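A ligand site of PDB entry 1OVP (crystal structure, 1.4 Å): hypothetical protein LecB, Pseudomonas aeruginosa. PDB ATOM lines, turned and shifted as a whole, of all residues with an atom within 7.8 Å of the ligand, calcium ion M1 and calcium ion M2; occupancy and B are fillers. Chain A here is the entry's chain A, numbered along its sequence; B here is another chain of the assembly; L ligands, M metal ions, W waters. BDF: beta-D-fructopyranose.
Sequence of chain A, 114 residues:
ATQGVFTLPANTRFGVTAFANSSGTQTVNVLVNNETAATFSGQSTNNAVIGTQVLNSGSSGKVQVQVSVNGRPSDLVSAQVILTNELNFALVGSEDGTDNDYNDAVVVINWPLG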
ATOM      1  N   ALA A  20      30.950   1.115  29.575  1.00  0.00           N
ATOM      2  CA  ALA A  20      29.722   1.789  29.968  1.00  0.00           C
ATOM      3  C   ALA A  20      29.962   2.826  31.063  1.00  0.00           C
ATOM      4  O   ALA A  20      30.754   2.602  31.981  1.00  0.00           O
ATOM      5  CB  ALA A  20      28.688   0.775  30.435  1.00  0.00           C
ATOM      6  N   ASN A  21      29.260   3.950  30.953  1.00  0.00           N
ATOM      7  CA  ASN A  21      29.339   5.062  31.914  1.00  0.00           C
ATOM      8  C   ASN A  21      27.971   5.731  31.958  1.00  0.00           C
ATOM      9  O   ASN A  21      27.793   6.846  31.465  1.00  0.00           O
ATOM     10  CB  ASN A  21      30.384   6.087  31.464  1.00  0.00           C
ATOM     11  CG  ASN A  21      31.801   5.571  31.565  1.00  0.00           C
ATOM     12  OD1 ASN A  21      32.363   5.486  32.657  1.00  0.00           O
ATOM     13  ND2 ASN A  21      32.380   5.194  30.426  1.00  0.00           N
ATOM     14  N   SER A  22      26.999   5.049  32.557  1.00  0.00           N
ATOM     15  CA  SER A  22      25.643   5.573  32.634  1.00  0.00           C
ATOM     16  C   SER A  22      24.801   4.733  33.584  1.00  0.00           C
ATOM     17  O   SER A  22      25.141   3.589  33.873  1.00  0.00           O
ATOM     18  CB  SER A  22      25.010   5.546  31.243  1.00  0.00           C
ATOM     19  OG  SER A  22      23.632   5.889  31.295  1.00  0.00           O
ATOM     20  N   SER A  23      23.701   5.300  34.062  1.00  0.00           N
ATOM     21  CA  SER A  23      22.812   4.564  34.948  1.00  0.00           C
ATOM     22  C   SER A  23      22.002   3.575  34.122  1.00  0.00           C
ATOM     23  O   SER A  23      21.555   2.560  34.635  1.00  0.00           O
ATOM     24  CB  SER A  23      21.861   5.529  35.668  1.00  0.00           C
ATOM     25  OG  SER A  23      21.004   6.177  34.747  1.00  0.00           O
ATOM     26  N   GLY A  24      21.831   3.886  32.843  1.00  0.00           N
ATOM     27  CA  GLY A  24      21.047   3.020  31.984  1.00  0.00           C
ATOM     28  C   GLY A  24      21.821   1.859  31.388  1.00  0.00           C
ATOM     29  O   GLY A  24      23.028   1.958  31.139  1.00  0.00           O
ATOM     30  N   THR A  25      21.131   0.750  31.173  1.00  0.00           N
ATOM     31  CA  THR A  25      21.736  -0.441  30.587  1.00  0.00           C
ATOM     32  C   THR A  25      22.004  -0.137  29.118  1.00  0.00           C
ATOM     33  O   THR A  25      21.109   0.261  28.378  1.00  0.00           O
ATOM     34  CB  THR A  25      20.791  -1.647  30.702  1.00  0.00           C
ATOM     35  OG1 THR A  25      20.582  -1.935  32.092  1.00  0.00           O
ATOM     36  CG2 THR A  25      21.378  -2.863  30.011  1.00  0.00           C
ATOM     37  N   GLN A  26      23.263  -0.315  28.710  1.00  0.00           N
ATOM     38  CA  GLN A  26      23.672  -0.037  27.351  1.00  0.00           C
ATOM     39  C   GLN A  26      23.622  -1.291  26.483  1.00  0.00           C
ATOM     40  O   GLN A  26      24.092  -2.350  26.888  1.00  0.00           O
ATOM     41  CB  GLN A  26      25.099   0.510  27.349  1.00  0.00           C
ATOM     42  CG  GLN A  26      25.304   1.691  28.287  1.00  0.00           C
ATOM     43  CD  GLN A  26      24.556   2.942  27.844  1.00  0.00           C
ATOM     44  OE1 GLN A  26      23.922   3.614  28.650  1.00  0.00           O
ATOM     45  NE2 GLN A  26      24.662   3.262  26.563  1.00  0.00           N
ATOM     46  N   GLN A  43      25.758  -2.645  32.283  1.00  0.00           N
ATOM     47  CA  GLN A  43      25.547  -1.380  32.986  1.00  0.00           C
ATOM     48  C   GLN A  43      26.716  -1.106  33.914  1.00  0.00           C
ATOM     49  O   GLN A  43      27.186  -1.998  34.619  1.00  0.00           O
ATOM     50  CB  GLN A  43      24.237  -1.443  33.782  1.00  0.00           C
ATOM     51  CG  GLN A  43      23.814  -0.158  34.497  1.00  0.00           C
ATOM     52  CD  GLN A  43      24.682   0.188  35.706  1.00  0.00           C
ATOM     53  OE1 GLN A  43      24.956  -0.673  36.540  1.00  0.00           O
ATOM     54  NE2 GLN A  43      25.070   1.444  35.819  1.00  0.00           N
ATOM     55  N   SER A  44      27.172   0.141  33.903  1.00  0.00           N
ATOM     56  CA  SER A  44      28.262   0.564  34.749  1.00  0.00           C
ATOM     57  C   SER A  44      28.393   2.077  34.698  1.00  0.00           C
ATOM     58  O   SER A  44      28.048   2.706  33.693  1.00  0.00           O
ATOM     59  CB  SER A  44      29.588  -0.046  34.286  1.00  0.00           C
ATOM     60  OG  SER A  44      30.683   0.477  35.030  1.00  0.00           O
ATOM     61  N   THR A  45      28.842   2.656  35.798  1.00  0.00           N
ATOM     62  CA  THR A  45      29.092   4.082  35.855  1.00  0.00           C
ATOM     63  C   THR A  45      30.584   4.271  36.157  1.00  0.00           C
ATOM     64  O   THR A  45      31.030   5.366  36.477  1.00  0.00           O
ATOM     65  CB  THR A  45      28.234   4.799  36.932  1.00  0.00           C
ATOM     66  OG1 THR A  45      28.270   4.070  38.161  1.00  0.00           O
ATOM     67  CG2 THR A  45      26.794   4.938  36.452  1.00  0.00           C
ATOM     68  N   VAL A  69      19.481   2.415  24.612  1.00  0.00           N
ATOM     69  CA  VAL A  69      19.174   2.207  26.010  1.00  0.00           C
ATOM     70  C   VAL A  69      17.673   1.991  26.068  1.00  0.00           C
ATOM     71  O   VAL A  69      16.890   2.850  25.674  1.00  0.00           O
ATOM     72  CB  VAL A  69      19.573   3.421  26.884  1.00  0.00           C
ATOM     73  CG1 VAL A  69      19.154   3.175  28.332  1.00  0.00           C
ATOM     74  CG2 VAL A  69      21.070   3.656  26.799  1.00  0.00           C
ATOM     75  N   SER A  94      28.654   7.843  22.753  1.00  0.00           N
ATOM     76  CA  SER A  94      27.203   7.900  22.663  1.00  0.00           C
ATOM     77  C   SER A  94      26.582   8.618  23.847  1.00  0.00           C
ATOM     78  O   SER A  94      27.108   8.566  24.955  1.00  0.00           O
ATOM     79  CB  SER A  94      26.624   6.489  22.542  1.00  0.00           C
ATOM     80  OG  SER A  94      26.914   5.727  23.690  1.00  0.00           O
ATOM     81  N   GLU A  95      25.470   9.297  23.601  1.00  0.00           N
ATOM     82  CA  GLU A  95      24.768  10.019  24.650  1.00  0.00           C
ATOM     83  C   GLU A  95      23.329   9.538  24.716  1.00  0.00           C
ATOM     84  O   GLU A  95      22.591   9.589  23.725  1.00  0.00           O
ATOM     85  CB  GLU A  95      24.809  11.516  24.367  1.00  0.00           C
ATOM     86  CG  GLU A  95      24.071  12.365  25.385  1.00  0.00           C
ATOM     87  CD  GLU A  95      24.542  12.127  26.801  1.00  0.00           C
ATOM     88  OE1 GLU A  95      25.763  12.205  27.044  1.00  0.00           O
ATOM     89  OE2 GLU A  95      23.692  11.878  27.680  1.00  0.00           O
ATOM     90  N   ASP A  96      22.937   9.064  25.895  1.00  0.00           N
ATOM     91  CA  ASP A  96      21.594   8.551  26.117  1.00  0.00           C
ATOM     92  C   ASP A  96      20.697   9.540  26.852  1.00  0.00           C
ATOM     93  O   ASP A  96      19.495   9.314  26.972  1.00  0.00           O
ATOM     94  CB  ASP A  96      21.632   7.236  26.923  1.00  0.00           C
ATOM     95  CG  ASP A  96      22.242   7.412  28.317  1.00  0.00           C
ATOM     96  OD1 ASP A  96      21.957   8.434  28.983  1.00  0.00           O
ATOM     97  OD2 ASP A  96      22.971   6.504  28.764  1.00  0.00           O
ATOM     98  N   GLY A  97      21.287  10.641  27.307  1.00  0.00           N
ATOM     99  CA  GLY A  97      20.508  11.609  28.050  1.00  0.00           C
ATOM    100  C   GLY A  97      20.680  13.075  27.718  1.00  0.00           C
ATOM    101  O   GLY A  97      20.689  13.468  26.552  1.00  0.00           O
ATOM    102  N   THR A  98      20.830  13.887  28.763  1.00  0.00           N
ATOM    103  CA  THR A  98      20.945  15.332  28.602  1.00  0.00           C
ATOM    104  C   THR A  98      22.239  15.991  29.053  1.00  0.00           C
ATOM    105  O   THR A  98      22.445  17.168  28.774  1.00  0.00           O
ATOM    106  CB  THR A  98      19.788  16.024  29.355  1.00  0.00           C
ATOM    107  OG1 THR A  98      19.852  15.666  30.740  1.00  0.00           O
ATOM    108  CG2 THR A  98      18.443  15.593  28.786  1.00  0.00           C
ATOM    109  N   ASP A  99      23.118  15.264  29.729  1.00  0.00           N
ATOM    110  CA  ASP A  99      24.344  15.896  30.206  1.00  0.00           C
ATOM    111  C   ASP A  99      25.441  16.039  29.150  1.00  0.00           C
ATOM    112  O   ASP A  99      26.409  16.770  29.344  1.00  0.00           O
ATOM    113  CB  ASP A  99      24.865  15.146  31.441  1.00  0.00           C
ATOM    114  CG  ASP A  99      25.408  13.776  31.120  1.00  0.00           C
ATOM    115  OD1 ASP A  99      25.121  13.255  30.028  1.00  0.00           O
ATOM    116  OD2 ASP A  99      26.123  13.219  31.982  1.00  0.00           O
ATOM    117  N   ASN A 100      25.268  15.350  28.026  1.00  0.00           N
ATOM    118  CA  ASN A 100      26.212  15.413  26.918  1.00  0.00           C
ATOM    119  C   ASN A 100      27.662  15.044  27.219  1.00  0.00           C
ATOM    120  O   ASN A 100      28.582  15.705  26.727  1.00  0.00           O
ATOM    121  CB  ASN A 100      26.175  16.788  26.255  1.00  0.00           C
ATOM    122  CG  ASN A 100      24.804  17.106  25.697  1.00  0.00           C
ATOM    123  OD1 ASN A 100      24.196  16.270  25.030  1.00  0.00           O
ATOM    124  ND2 ASN A 100      24.327  18.314  25.947  1.00  0.00           N
ATOM    125  N   ASP A 101      27.877  14.023  28.028  1.00  0.00           N
ATOM    126  CA  ASP A 101      29.240  13.605  28.272  1.00  0.00           C
ATOM    127  C   ASP A 101      29.661  12.611  27.185  1.00  0.00           C
ATOM    128  O   ASP A 101      30.847  12.348  27.010  1.00  0.00           O
ATOM    129  CB  ASP A 101      29.425  13.038  29.706  1.00  0.00           C
ATOM    130  CG  ASP A 101      28.523  11.862  30.022  1.00  0.00           C
ATOM    131  OD1 ASP A 101      27.652  11.483  29.216  1.00  0.00           O
ATOM    132  OD2 ASP A 101      28.694  11.327  31.144  1.00  0.00           O
ATOM    133  N   TYR A 102      28.683  12.113  26.426  1.00  0.00           N
ATOM    134  CA  TYR A 102      28.915  11.193  25.310  1.00  0.00           C
ATOM    135  C   TYR A 102      29.782   9.984  25.611  1.00  0.00           C
ATOM    136  O   TYR A 102      30.456   9.446  24.726  1.00  0.00           O
ATOM    137  CB  TYR A 102      29.467  11.974  24.112  1.00  0.00           C
ATOM    138  CG  TYR A 102      28.375  12.667  23.326  1.00  0.00           C
ATOM    139  CD1 TYR A 102      27.733  12.006  22.277  1.00  0.00           C
ATOM    140  CD2 TYR A 102      27.899  13.922  23.703  1.00  0.00           C
ATOM    141  CE1 TYR A 102      26.639  12.572  21.625  1.00  0.00           C
ATOM    142  CE2 TYR A 102      26.816  14.500  23.053  1.00  0.00           C
ATOM    143  CZ  TYR A 102      26.189  13.813  22.024  1.00  0.00           C
ATOM    144  OH  TYR A 102      25.088  14.359  21.412  1.00  0.00           O
ATOM    145  N   ASN A 103      29.745   9.527  26.853  1.00  0.00           N
ATOM    146  CA  ASN A 103      30.535   8.388  27.270  1.00  0.00           C
ATOM    147  C   ASN A 103      29.631   7.276  27.801  1.00  0.00           C
ATOM    148  O   ASN A 103      30.114   6.272  28.314  1.00  0.00           O
ATOM    149  CB  ASN A 103      31.472   8.803  28.409  1.00  0.00           C
ATOM    150  CG  ASN A 103      30.726   9.049  29.709  1.00  0.00           C
ATOM    151  OD1 ASN A 103      29.495   9.021  29.744  1.00  0.00           O
ATOM    152  ND2 ASN A 103      31.472   9.290  30.780  1.00  0.00           N
ATOM    153  N   ASP A 104      28.330   7.459  27.655  1.00  0.00           N
ATOM    154  CA  ASP A 104      27.389   6.489  28.207  1.00  0.00           C
ATOM    155  C   ASP A 104      27.708   5.075  27.760  1.00  0.00           C
ATOM    156  O   ASP A 104      27.602   4.124  28.527  1.00  0.00           O
ATOM    157  CB  ASP A 104      25.964   6.935  27.896  1.00  0.00           C
ATOM    158  CG  ASP A 104      25.698   8.341  28.433  1.00  0.00           C
ATOM    159  OD1 ASP A 104      26.190   8.651  29.532  1.00  0.00           O
ATOM    160  OD2 ASP A 104      25.003   9.130  27.759  1.00  0.00           O
ATOM    161  N   ALA A 105      28.131   4.967  26.505  1.00  0.00           N
ATOM    162  CA  ALA A 105      28.603   3.719  25.921  1.00  0.00           C
ATOM    163  C   ALA A 105      29.743   4.210  25.027  1.00  0.00           C
ATOM    164  O   ALA A 105      29.542   5.067  24.177  1.00  0.00           O
ATOM    165  CB  ALA A 105      27.519   3.062  25.089  1.00  0.00           C
ATOM    166  N   PRO B 112      35.684  11.775  29.699  1.00  0.00           N
ATOM    167  CA  PRO B 112      35.351  11.593  31.105  1.00  0.00           C
ATOM    168  C   PRO B 112      34.668  10.250  31.355  1.00  0.00           C
ATOM    169  O   PRO B 112      34.238   9.565  30.423  1.00  0.00           O
ATOM    170  CB  PRO B 112      34.405  12.750  31.377  1.00  0.00           C
ATOM    171  CG  PRO B 112      33.621  12.778  30.093  1.00  0.00           C
ATOM    172  CD  PRO B 112      34.769  12.780  29.103  1.00  0.00           C
ATOM    173  N   LEU B 113      34.555   9.895  32.639  1.00  0.00           N
ATOM    174  CA  LEU B 113      33.883   8.666  33.040  1.00  0.00           C
ATOM    175  C   LEU B 113      32.623   9.031  33.822  1.00  0.00           C
ATOM    176  O   LEU B 113      32.380  10.194  34.102  1.00  0.00           O
ATOM    177  CB  LEU B 113      34.797   7.834  33.958  1.00  0.00           C
ATOM    178  CG  LEU B 113      36.178   7.442  33.427  1.00  0.00           C
ATOM    179  CD1 LEU B 113      36.858   6.529  34.434  1.00  0.00           C
ATOM    180  CD2 LEU B 113      36.048   6.740  32.083  1.00  0.00           C
ATOM    181  N   GLY B 114      31.822   8.018  34.145  1.00  0.00           N
ATOM    182  CA  GLY B 114      30.613   8.215  34.925  1.00  0.00           C
ATOM    183  C   GLY B 114      29.342   8.558  34.165  1.00  0.00           C
ATOM    184  O   GLY B 114      29.412   8.943  32.989  1.00  0.00           O
ATOM    185  OXT GLY B 114      28.261   8.456  34.798  1.00  0.00           O
HETATM  186  C1  BDF L   1      21.408   8.237  32.314  1.00  0.00           C
HETATM  187  C2  BDF L   1      22.671   9.254  32.684  1.00  0.00           C
HETATM  188  C3  BDF L   1      23.780   9.528  31.668  1.00  0.00           C
HETATM  189  C4  BDF L   1      24.897  10.346  32.451  1.00  0.00           C
HETATM  190  C5  BDF L   1      25.471   9.716  33.691  1.00  0.00           C
HETATM  191  C6  BDF L   1      24.288   9.270  34.580  1.00  0.00           C
HETATM  192  O1  BDF L   1      20.340   8.244  33.341  1.00  0.00           O
HETATM  193  O2  BDF L   1      22.261  10.457  33.147  1.00  0.00           O
HETATM  194  O3  BDF L   1      23.262  10.329  30.532  1.00  0.00           O
HETATM  195  O4  BDF L   1      25.927  10.817  31.630  1.00  0.00           O
HETATM  196  O5  BDF L   1      26.388   8.653  33.199  1.00  0.00           O
HETATM  197  O6  BDF L   1      23.344   8.550  33.760  1.00  0.00           O
HETATM  198 CA    CA M   1      25.337  11.069  29.168  1.00  0.00          CA
HETATM  199 CA    CA M   2      27.730   9.183  31.255  1.00  0.00          CA
HETATM  200  O   HOH W   1      21.888  13.445  34.013  1.00  0.00           O
HETATM  201  O   HOH W   2      21.040  10.629  35.668  1.00  0.00           O
HETATM  202  O   HOH W   3      22.184  12.800  31.213  1.00  0.00           O
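Four residues have an atom within 4 Å of calcium ion M1: Glu 95, Asp 99, Asp 101 and Asp 104.
The backbone NH of Asn 103 lies within hydrogen-bond range of the backbone carbonyl oxygen of Ser 94 (3.4 Å).
The backbone NH (N) of Asn 21 sits close to the backbone carbonyl oxygen (O) of Ser 44 (3.2 Å).
N of Gly 97 sits close to OE2 of Glu 95.
The backbone NH of Asn 100 sits close to the side-chain carboxylate of Glu 95 (3.3 Å).
The backbone NH of Asp 96 lies close to the side-chain carboxylate of Asp 104 (2.8 Å).
OD2 of Asp 96 lies close to OE1 of Gln 26 (3.0 Å).
The backbone NH of Ser 22 sits at hydrogen-bond distance from the backbone carbonyl oxygen of Ser 44, 2.8 Å away.
The side-chain amide nitrogen (NE2) of Gln 43 is in hydrogen-bond range of the backbone carbonyl oxygen (O) of Ser 22, at 2.9 Å.
Water W3 lies within hydrogen-bond range of the backbone NH (N) of Thr 98 (3.0 Å), the backbone NH (N) of Asp 99 (3.0 Å) and an oxygen (O2) of the ligand (3.0 Å).
Calcium ion M2 is bound by the side-chain amide oxygen (OD1) of Asn 103, the backbone carbonyl oxygen (O) of Asn 21, the side-chain carboxylate (OD2) of Asp 101, the side-chain carboxylate (OD1) of Asp 104, an oxygen (O5) of the ligand, the chain-end carboxylate (O) of Gly 114 of chain B and an oxygen (O4) of the ligand.
Calcium ion M2 has seven donor atoms within binding distance.
Slightly farther from calcium ion M2 lies the side-chain carboxylate (OD1) of Asp 101 (3.1 Å).
N of Ser 23 sits at hydrogen-bond distance from O6 of the ligand (3.3 Å).
OG of Ser 23 is in hydrogen-bond range of O1 of the ligand (2.6 Å).
An oxygen (O3) of the ligand lies close to the side-chain carboxylate (OD1) of Asp 96 (2.8 Å).
CA of Ser 22 touches O5 of the ligand (3.2 Å).
Gly 97 touches the ligand.
Ten residues have an atom within 4 Å of the ligand: Asn 21, Ser 22, Ser 23, Glu 95, Asp 96, Gly 97, Asp 99, Asp 101, Asp 104 and Gly 114 of chain B.
The nearest printed residue that does not touch the ligand is Gly 24 (4.4 Å).
Calcium ion M1 is bound by OD1 of Asp 101 (2.4 Å), OD1 of Asp 99 (2.4 Å), OE2 of Glu 95 (2.4 Å), OD2 of Asp 104 (2.4 Å), OE1 of Glu 95 (2.4 Å), O4 of the ligand (2.5 Å), OD1 of Asp 104 (2.6 Å) and O3 of the ligand (2.6 Å).
Calcium ion M1 has eight donor atoms within binding distance.
Of the 26 residues printed, 5 come within 4 Å of calcium ion M2.
The nearest printed residue that does not touch calcium ion M2 is Ser 22 (4.4 Å).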
